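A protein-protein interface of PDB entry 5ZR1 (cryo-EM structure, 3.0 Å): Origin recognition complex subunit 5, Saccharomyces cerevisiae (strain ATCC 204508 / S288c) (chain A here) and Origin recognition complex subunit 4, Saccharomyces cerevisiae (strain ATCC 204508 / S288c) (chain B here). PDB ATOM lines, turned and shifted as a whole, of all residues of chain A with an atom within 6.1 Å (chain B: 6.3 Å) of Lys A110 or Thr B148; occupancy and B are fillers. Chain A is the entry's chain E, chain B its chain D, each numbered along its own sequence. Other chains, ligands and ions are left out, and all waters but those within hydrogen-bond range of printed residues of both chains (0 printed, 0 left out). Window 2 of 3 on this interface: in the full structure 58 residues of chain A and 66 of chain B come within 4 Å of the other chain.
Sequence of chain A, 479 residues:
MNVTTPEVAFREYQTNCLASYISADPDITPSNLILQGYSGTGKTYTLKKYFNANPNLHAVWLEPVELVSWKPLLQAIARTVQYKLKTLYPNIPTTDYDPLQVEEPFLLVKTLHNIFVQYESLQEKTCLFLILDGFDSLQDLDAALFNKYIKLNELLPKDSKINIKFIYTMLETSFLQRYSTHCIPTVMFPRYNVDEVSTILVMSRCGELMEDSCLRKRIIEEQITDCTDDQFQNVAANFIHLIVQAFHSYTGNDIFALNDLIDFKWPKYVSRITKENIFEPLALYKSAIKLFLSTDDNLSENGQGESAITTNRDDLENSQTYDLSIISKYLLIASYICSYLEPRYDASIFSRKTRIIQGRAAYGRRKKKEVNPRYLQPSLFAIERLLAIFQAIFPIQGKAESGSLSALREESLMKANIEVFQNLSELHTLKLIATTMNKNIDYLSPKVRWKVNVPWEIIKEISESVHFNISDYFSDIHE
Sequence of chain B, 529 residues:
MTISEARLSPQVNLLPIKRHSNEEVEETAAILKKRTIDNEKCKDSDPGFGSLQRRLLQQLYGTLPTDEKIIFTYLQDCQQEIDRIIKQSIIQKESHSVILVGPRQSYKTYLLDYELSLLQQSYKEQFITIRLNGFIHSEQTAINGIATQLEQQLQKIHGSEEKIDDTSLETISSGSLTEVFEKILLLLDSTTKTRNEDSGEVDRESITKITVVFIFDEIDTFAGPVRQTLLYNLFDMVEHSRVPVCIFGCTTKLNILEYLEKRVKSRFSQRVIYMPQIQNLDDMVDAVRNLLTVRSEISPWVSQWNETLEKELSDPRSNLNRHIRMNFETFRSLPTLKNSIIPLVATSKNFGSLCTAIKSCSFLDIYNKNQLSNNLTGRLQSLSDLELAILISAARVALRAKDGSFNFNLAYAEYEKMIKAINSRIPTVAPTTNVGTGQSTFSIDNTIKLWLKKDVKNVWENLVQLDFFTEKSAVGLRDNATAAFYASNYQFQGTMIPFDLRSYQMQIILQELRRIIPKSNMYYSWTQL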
ATOM      1  N   PRO A 105      17.748  17.850  35.288  1.00  0.00           N
ATOM      2  CA  PRO A 105      19.142  17.517  35.604  1.00  0.00           C
ATOM      3  C   PRO A 105      19.817  16.668  34.542  1.00  0.00           C
ATOM      4  O   PRO A 105      21.051  16.667  34.475  1.00  0.00           O
ATOM      5  CB  PRO A 105      19.031  16.768  36.933  1.00  0.00           C
ATOM      6  CG  PRO A 105      17.778  17.269  37.524  1.00  0.00           C
ATOM      7  CD  PRO A 105      16.841  17.479  36.385  1.00  0.00           C
ATOM      8  N   PHE A 106      19.058  15.940  33.721  1.00  0.00           N
ATOM      9  CA  PHE A 106      19.664  15.194  32.624  1.00  0.00           C
ATOM     10  C   PHE A 106      19.942  16.077  31.417  1.00  0.00           C
ATOM     11  O   PHE A 106      20.947  15.880  30.726  1.00  0.00           O
ATOM     12  CB  PHE A 106      18.784  14.022  32.208  1.00  0.00           C
ATOM     13  CG  PHE A 106      19.237  13.368  30.938  1.00  0.00           C
ATOM     14  CD1 PHE A 106      20.440  12.676  30.895  1.00  0.00           C
ATOM     15  CD2 PHE A 106      18.480  13.467  29.780  1.00  0.00           C
ATOM     16  CE1 PHE A 106      20.877  12.083  29.725  1.00  0.00           C
ATOM     17  CE2 PHE A 106      18.912  12.877  28.606  1.00  0.00           C
ATOM     18  CZ  PHE A 106      20.115  12.187  28.580  1.00  0.00           C
ATOM     19  N   LEU A 107      19.069  17.047  31.140  1.00  0.00           N
ATOM     20  CA  LEU A 107      19.309  17.950  30.022  1.00  0.00           C
ATOM     21  C   LEU A 107      20.507  18.854  30.257  1.00  0.00           C
ATOM     22  O   LEU A 107      21.042  19.402  29.294  1.00  0.00           O
ATOM     23  CB  LEU A 107      18.079  18.799  29.742  1.00  0.00           C
ATOM     24  CG  LEU A 107      16.870  18.048  29.204  1.00  0.00           C
ATOM     25  CD1 LEU A 107      15.724  18.998  29.074  1.00  0.00           C
ATOM     26  CD2 LEU A 107      17.178  17.415  27.871  1.00  0.00           C
ATOM     27  N   LEU A 108      20.932  19.027  31.508  1.00  0.00           N
ATOM     28  CA  LEU A 108      22.237  19.617  31.762  1.00  0.00           C
ATOM     29  C   LEU A 108      23.346  18.679  31.312  1.00  0.00           C
ATOM     30  O   LEU A 108      24.305  19.108  30.665  1.00  0.00           O
ATOM     31  CB  LEU A 108      22.390  19.953  33.243  1.00  0.00           C
ATOM     32  CG  LEU A 108      23.721  20.639  33.534  1.00  0.00           C
ATOM     33  CD1 LEU A 108      23.773  21.984  32.841  1.00  0.00           C
ATOM     34  CD2 LEU A 108      23.975  20.769  35.014  1.00  0.00           C
ATOM     35  N   VAL A 109      23.218  17.388  31.636  1.00  0.00           N
ATOM     36  CA  VAL A 109      24.234  16.398  31.280  1.00  0.00           C
ATOM     37  C   VAL A 109      24.327  16.241  29.768  1.00  0.00           C
ATOM     38  O   VAL A 109      25.423  16.115  29.211  1.00  0.00           O
ATOM     39  CB  VAL A 109      23.930  15.060  31.982  1.00  0.00           C
ATOM     40  CG1 VAL A 109      24.895  13.969  31.559  1.00  0.00           C
ATOM     41  CG2 VAL A 109      23.985  15.240  33.475  1.00  0.00           C
ATOM     42  N   LYS A 110      23.189  16.302  29.074  1.00  0.00           N
ATOM     43  CA  LYS A 110      23.213  16.220  27.617  1.00  0.00           C
ATOM     44  C   LYS A 110      23.800  17.484  26.996  1.00  0.00           C
ATOM     45  O   LYS A 110      24.533  17.409  26.005  1.00  0.00           O
ATOM     46  CB  LYS A 110      21.807  15.955  27.083  1.00  0.00           C
ATOM     47  CG  LYS A 110      21.759  15.725  25.584  1.00  0.00           C
ATOM     48  CD  LYS A 110      20.389  15.281  25.119  1.00  0.00           C
ATOM     49  CE  LYS A 110      19.407  16.424  25.091  1.00  0.00           C
ATOM     50  NZ  LYS A 110      19.729  17.395  24.015  1.00  0.00           N
ATOM     51  N   THR A 111      23.504  18.651  27.575  1.00  0.00           N
ATOM     52  CA  THR A 111      24.061  19.901  27.067  1.00  0.00           C
ATOM     53  C   THR A 111      25.555  19.996  27.341  1.00  0.00           C
ATOM     54  O   THR A 111      26.323  20.392  26.458  1.00  0.00           O
ATOM     55  CB  THR A 111      23.316  21.087  27.675  1.00  0.00           C
ATOM     56  OG1 THR A 111      21.947  21.027  27.268  1.00  0.00           O
ATOM     57  CG2 THR A 111      23.903  22.410  27.230  1.00  0.00           C
ATOM     58  N   LEU A 112      25.990  19.613  28.545  1.00  0.00           N
ATOM     59  CA  LEU A 112      27.419  19.593  28.839  1.00  0.00           C
ATOM     60  C   LEU A 112      28.146  18.538  28.018  1.00  0.00           C
ATOM     61  O   LEU A 112      29.312  18.731  27.670  1.00  0.00           O
ATOM     62  CB  LEU A 112      27.659  19.356  30.328  1.00  0.00           C
ATOM     63  CG  LEU A 112      27.214  20.459  31.287  1.00  0.00           C
ATOM     64  CD1 LEU A 112      27.419  20.018  32.719  1.00  0.00           C
ATOM     65  CD2 LEU A 112      27.941  21.750  31.006  1.00  0.00           C
ATOM     66  N   HIS A 113      27.476  17.435  27.679  1.00  0.00           N
ATOM     67  CA  HIS A 113      28.069  16.473  26.757  1.00  0.00           C
ATOM     68  C   HIS A 113      28.206  17.050  25.357  1.00  0.00           C
ATOM     69  O   HIS A 113      29.163  16.729  24.652  1.00  0.00           O
ATOM     70  CB  HIS A 113      27.240  15.190  26.708  1.00  0.00           C
ATOM     71  CG  HIS A 113      27.821  14.128  25.831  1.00  0.00           C
ATOM     72  ND1 HIS A 113      28.885  13.343  26.218  1.00  0.00           N
ATOM     73  CD2 HIS A 113      27.499  13.733  24.577  1.00  0.00           C
ATOM     74  CE1 HIS A 113      29.184  12.501  25.246  1.00  0.00           C
ATOM     75  NE2 HIS A 113      28.360  12.718  24.238  1.00  0.00           N
ATOM     76  N   ASN A 114      27.277  17.910  24.939  1.00  0.00           N
ATOM     77  CA  ASN A 114      27.379  18.505  23.614  1.00  0.00           C
ATOM     78  C   ASN A 114      28.386  19.646  23.570  1.00  0.00           C
ATOM     79  O   ASN A 114      29.023  19.857  22.534  1.00  0.00           O
ATOM     80  CB  ASN A 114      26.016  19.007  23.146  1.00  0.00           C
ATOM     81  CG  ASN A 114      25.055  17.883  22.841  1.00  0.00           C
ATOM     82  OD1 ASN A 114      25.445  16.849  22.302  1.00  0.00           O
ATOM     83  ND2 ASN A 114      23.785  18.087  23.164  1.00  0.00           N
ATOM     84  N   ILE A 115      28.528  20.398  24.663  1.00  0.00           N
ATOM     85  CA  ILE A 115      29.505  21.483  24.705  1.00  0.00           C
ATOM     86  C   ILE A 115      30.923  20.926  24.713  1.00  0.00           C
ATOM     87  O   ILE A 115      31.818  21.455  24.047  1.00  0.00           O
ATOM     88  CB  ILE A 115      29.230  22.388  25.925  1.00  0.00           C
ATOM     89  CG1 ILE A 115      27.923  23.155  25.747  1.00  0.00           C
ATOM     90  CG2 ILE A 115      30.349  23.375  26.175  1.00  0.00           C
ATOM     91  CD1 ILE A 115      27.448  23.822  27.009  1.00  0.00           C
ATOM     92  N   ILE B 143      13.658   7.556  30.059  1.00  0.00           N
ATOM     93  CA  ILE B 143      13.329   7.145  28.701  1.00  0.00           C
ATOM     94  C   ILE B 143      14.138   7.953  27.698  1.00  0.00           C
ATOM     95  O   ILE B 143      14.655   7.413  26.715  1.00  0.00           O
ATOM     96  CB  ILE B 143      11.818   7.289  28.459  1.00  0.00           C
ATOM     97  CG1 ILE B 143      11.035   6.540  29.538  1.00  0.00           C
ATOM     98  CG2 ILE B 143      11.447   6.779  27.088  1.00  0.00           C
ATOM     99  CD1 ILE B 143      11.362   5.079  29.625  1.00  0.00           C
ATOM    100  N   ASN B 144      14.280   9.256  27.942  1.00  0.00           N
ATOM    101  CA  ASN B 144      15.104  10.091  27.079  1.00  0.00           C
ATOM    102  C   ASN B 144      16.583   9.810  27.283  1.00  0.00           C
ATOM    103  O   ASN B 144      17.381  10.009  26.365  1.00  0.00           O
ATOM    104  CB  ASN B 144      14.821  11.565  27.348  1.00  0.00           C
ATOM    105  CG  ASN B 144      13.429  11.969  26.951  1.00  0.00           C
ATOM    106  OD1 ASN B 144      12.936  11.583  25.896  1.00  0.00           O
ATOM    107  ND2 ASN B 144      12.775  12.741  27.806  1.00  0.00           N
ATOM    108  N   GLY B 145      16.963   9.355  28.477  1.00  0.00           N
ATOM    109  CA  GLY B 145      18.359   9.074  28.744  1.00  0.00           C
ATOM    110  C   GLY B 145      18.850   7.804  28.089  1.00  0.00           C
ATOM    111  O   GLY B 145      20.019   7.713  27.715  1.00  0.00           O
ATOM    112  N   ILE B 146      17.981   6.803  27.959  1.00  0.00           N
ATOM    113  CA  ILE B 146      18.356   5.587  27.246  1.00  0.00           C
ATOM    114  C   ILE B 146      18.504   5.875  25.760  1.00  0.00           C
ATOM    115  O   ILE B 146      19.510   5.513  25.141  1.00  0.00           O
ATOM    116  CB  ILE B 146      17.330   4.470  27.507  1.00  0.00           C
ATOM    117  CG1 ILE B 146      17.383   4.032  28.967  1.00  0.00           C
ATOM    118  CG2 ILE B 146      17.581   3.283  26.608  1.00  0.00           C
ATOM    119  CD1 ILE B 146      16.219   3.178  29.381  1.00  0.00           C
ATOM    120  N   ALA B 147      17.526   6.576  25.182  1.00  0.00           N
ATOM    121  CA  ALA B 147      17.493   6.788  23.737  1.00  0.00           C
ATOM    122  C   ALA B 147      18.580   7.739  23.266  1.00  0.00           C
ATOM    123  O   ALA B 147      19.067   7.606  22.139  1.00  0.00           O
ATOM    124  CB  ALA B 147      16.127   7.319  23.328  1.00  0.00           C
ATOM    125  N   THR B 148      18.958   8.710  24.097  1.00  0.00           N
ATOM    126  CA  THR B 148      20.069   9.588  23.749  1.00  0.00           C
ATOM    127  C   THR B 148      21.387   8.830  23.775  1.00  0.00           C
ATOM    128  O   THR B 148      22.208   8.965  22.863  1.00  0.00           O
ATOM    129  CB  THR B 148      20.115  10.777  24.704  1.00  0.00           C
ATOM    130  OG1 THR B 148      18.866  11.472  24.652  1.00  0.00           O
ATOM    131  CG2 THR B 148      21.212  11.731  24.310  1.00  0.00           C
ATOM    132  N   GLN B 149      21.590   7.998  24.794  1.00  0.00           N
ATOM    133  CA  GLN B 149      22.824   7.235  24.889  1.00  0.00           C
ATOM    134  C   GLN B 149      22.845   6.049  23.938  1.00  0.00           C
ATOM    135  O   GLN B 149      23.928   5.621  23.544  1.00  0.00           O
ATOM    136  CB  GLN B 149      23.045   6.755  26.319  1.00  0.00           C
ATOM    137  CG  GLN B 149      23.231   7.866  27.316  1.00  0.00           C
ATOM    138  CD  GLN B 149      23.422   7.348  28.714  1.00  0.00           C
ATOM    139  OE1 GLN B 149      23.490   6.145  28.934  1.00  0.00           O
ATOM    140  NE2 GLN B 149      23.469   8.253  29.679  1.00  0.00           N
ATOM    141  N   LEU B 150      21.683   5.495  23.569  1.00  0.00           N
ATOM    142  CA  LEU B 150      21.659   4.459  22.536  1.00  0.00           C
ATOM    143  C   LEU B 150      22.151   4.996  21.201  1.00  0.00           C
ATOM    144  O   LEU B 150      22.996   4.376  20.551  1.00  0.00           O
ATOM    145  CB  LEU B 150      20.259   3.871  22.363  1.00  0.00           C
ATOM    146  CG  LEU B 150      19.715   2.791  23.292  1.00  0.00           C
ATOM    147  CD1 LEU B 150      18.257   2.569  22.980  1.00  0.00           C
ATOM    148  CD2 LEU B 150      20.482   1.511  23.077  1.00  0.00           C
ATOM    149  N   GLU B 151      21.651   6.157  20.783  1.00  0.00           N
ATOM    150  CA  GLU B 151      22.012   6.640  19.461  1.00  0.00           C
ATOM    151  C   GLU B 151      23.419   7.212  19.400  1.00  0.00           C
ATOM    152  O   GLU B 151      23.982   7.270  18.309  1.00  0.00           O
ATOM    153  CB  GLU B 151      21.027   7.699  18.965  1.00  0.00           C
ATOM    154  CG  GLU B 151      21.107   9.026  19.675  1.00  0.00           C
ATOM    155  CD  GLU B 151      20.203  10.059  19.049  1.00  0.00           C
ATOM    156  OE1 GLU B 151      19.508   9.715  18.071  1.00  0.00           O
ATOM    157  OE2 GLU B 151      20.193  11.212  19.527  1.00  0.00           O
ATOM    158  N   GLN B 152      24.011   7.618  20.524  1.00  0.00           N
ATOM    159  CA  GLN B 152      25.357   8.170  20.464  1.00  0.00           C
ATOM    160  C   GLN B 152      26.429   7.136  20.769  1.00  0.00           C
ATOM    161  O   GLN B 152      27.595   7.356  20.424  1.00  0.00           O
ATOM    162  CB  GLN B 152      25.500   9.364  21.415  1.00  0.00           C
ATOM    163  CG  GLN B 152      25.540   9.025  22.888  1.00  0.00           C
ATOM    164  CD  GLN B 152      25.582  10.263  23.760  1.00  0.00           C
ATOM    165  OE1 GLN B 152      25.545  11.386  23.262  1.00  0.00           O
ATOM    166  NE2 GLN B 152      25.684  10.064  25.068  1.00  0.00           N
ATOM    167  N   GLN B 153      26.071   6.017  21.401  1.00  0.00           N
ATOM    168  CA  GLN B 153      26.993   4.894  21.490  1.00  0.00           C
ATOM    169  C   GLN B 153      27.040   4.098  20.194  1.00  0.00           C
ATOM    170  O   GLN B 153      28.074   3.500  19.880  1.00  0.00           O
ATOM    171  CB  GLN B 153      26.611   3.966  22.644  1.00  0.00           C
ATOM    172  CG  GLN B 153      26.882   4.492  24.041  1.00  0.00           C
ATOM    173  CD  GLN B 153      28.348   4.527  24.378  1.00  0.00           C
ATOM    174  OE1 GLN B 153      29.101   3.630  24.008  1.00  0.00           O
ATOM    175  NE2 GLN B 153      28.764   5.560  25.096  1.00  0.00           N
ATOM    176  N   SER B 173      16.149   8.962  19.141  1.00  0.00           N
ATOM    177  CA  SER B 173      15.855   9.846  20.259  1.00  0.00           C
ATOM    178  C   SER B 173      14.805  10.905  19.954  1.00  0.00           C
ATOM    179  O   SER B 173      14.321  11.552  20.887  1.00  0.00           O
ATOM    180  CB  SER B 173      17.132  10.537  20.727  1.00  0.00           C
ATOM    181  OG  SER B 173      16.855  11.459  21.764  1.00  0.00           O
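OE1 of Gln B152 is in hydrogen-bond range of NE2 of His A113 (3.3 Å).
Among the printed residues, merely in contact across the chains: Phe A106 with Gly B145 (3.6 Å), Lys A110 with Thr B148 (3.7 Å) and Phe A106 with Asn B144 (3.9 Å).
Printed residues of chain B within 4 Å of Phe A106: Asn B144 and Gly B145.
Of the printed residues of chain B, His A113 touches Gln B152.
Of the printed residues of chain A, Asn B144 touches Phe A106.
Of the printed residues of chain A, Gly B145 touches Phe A106.
Thr B148 touches just one residue of chain A: Lys A110 (3.7 Å).
Of the printed residues of chain A, Gln B152 touches His A113.
The nearest residue of chain A that does not touch Thr B148 is Phe A106 (4.1 Å).
The nearest printed residue of chain A that does not touch Gly B145 is Lys A110 (7.5 Å).
The side-chain amide nitrogen of Asn A114 is in hydrogen-bond range of the backbone carbonyl oxygen of Lys A110, at 3.0 Å.
OG1 of Thr B148 is in hydrogen-bond range of O of Asn B144 (2.7 Å).
Hydrophobic or aromatic side chains of chain A that line the printed part of chain B: Phe A106 and His A113.
Among the printed residues, 4 pairs touch across the chains.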
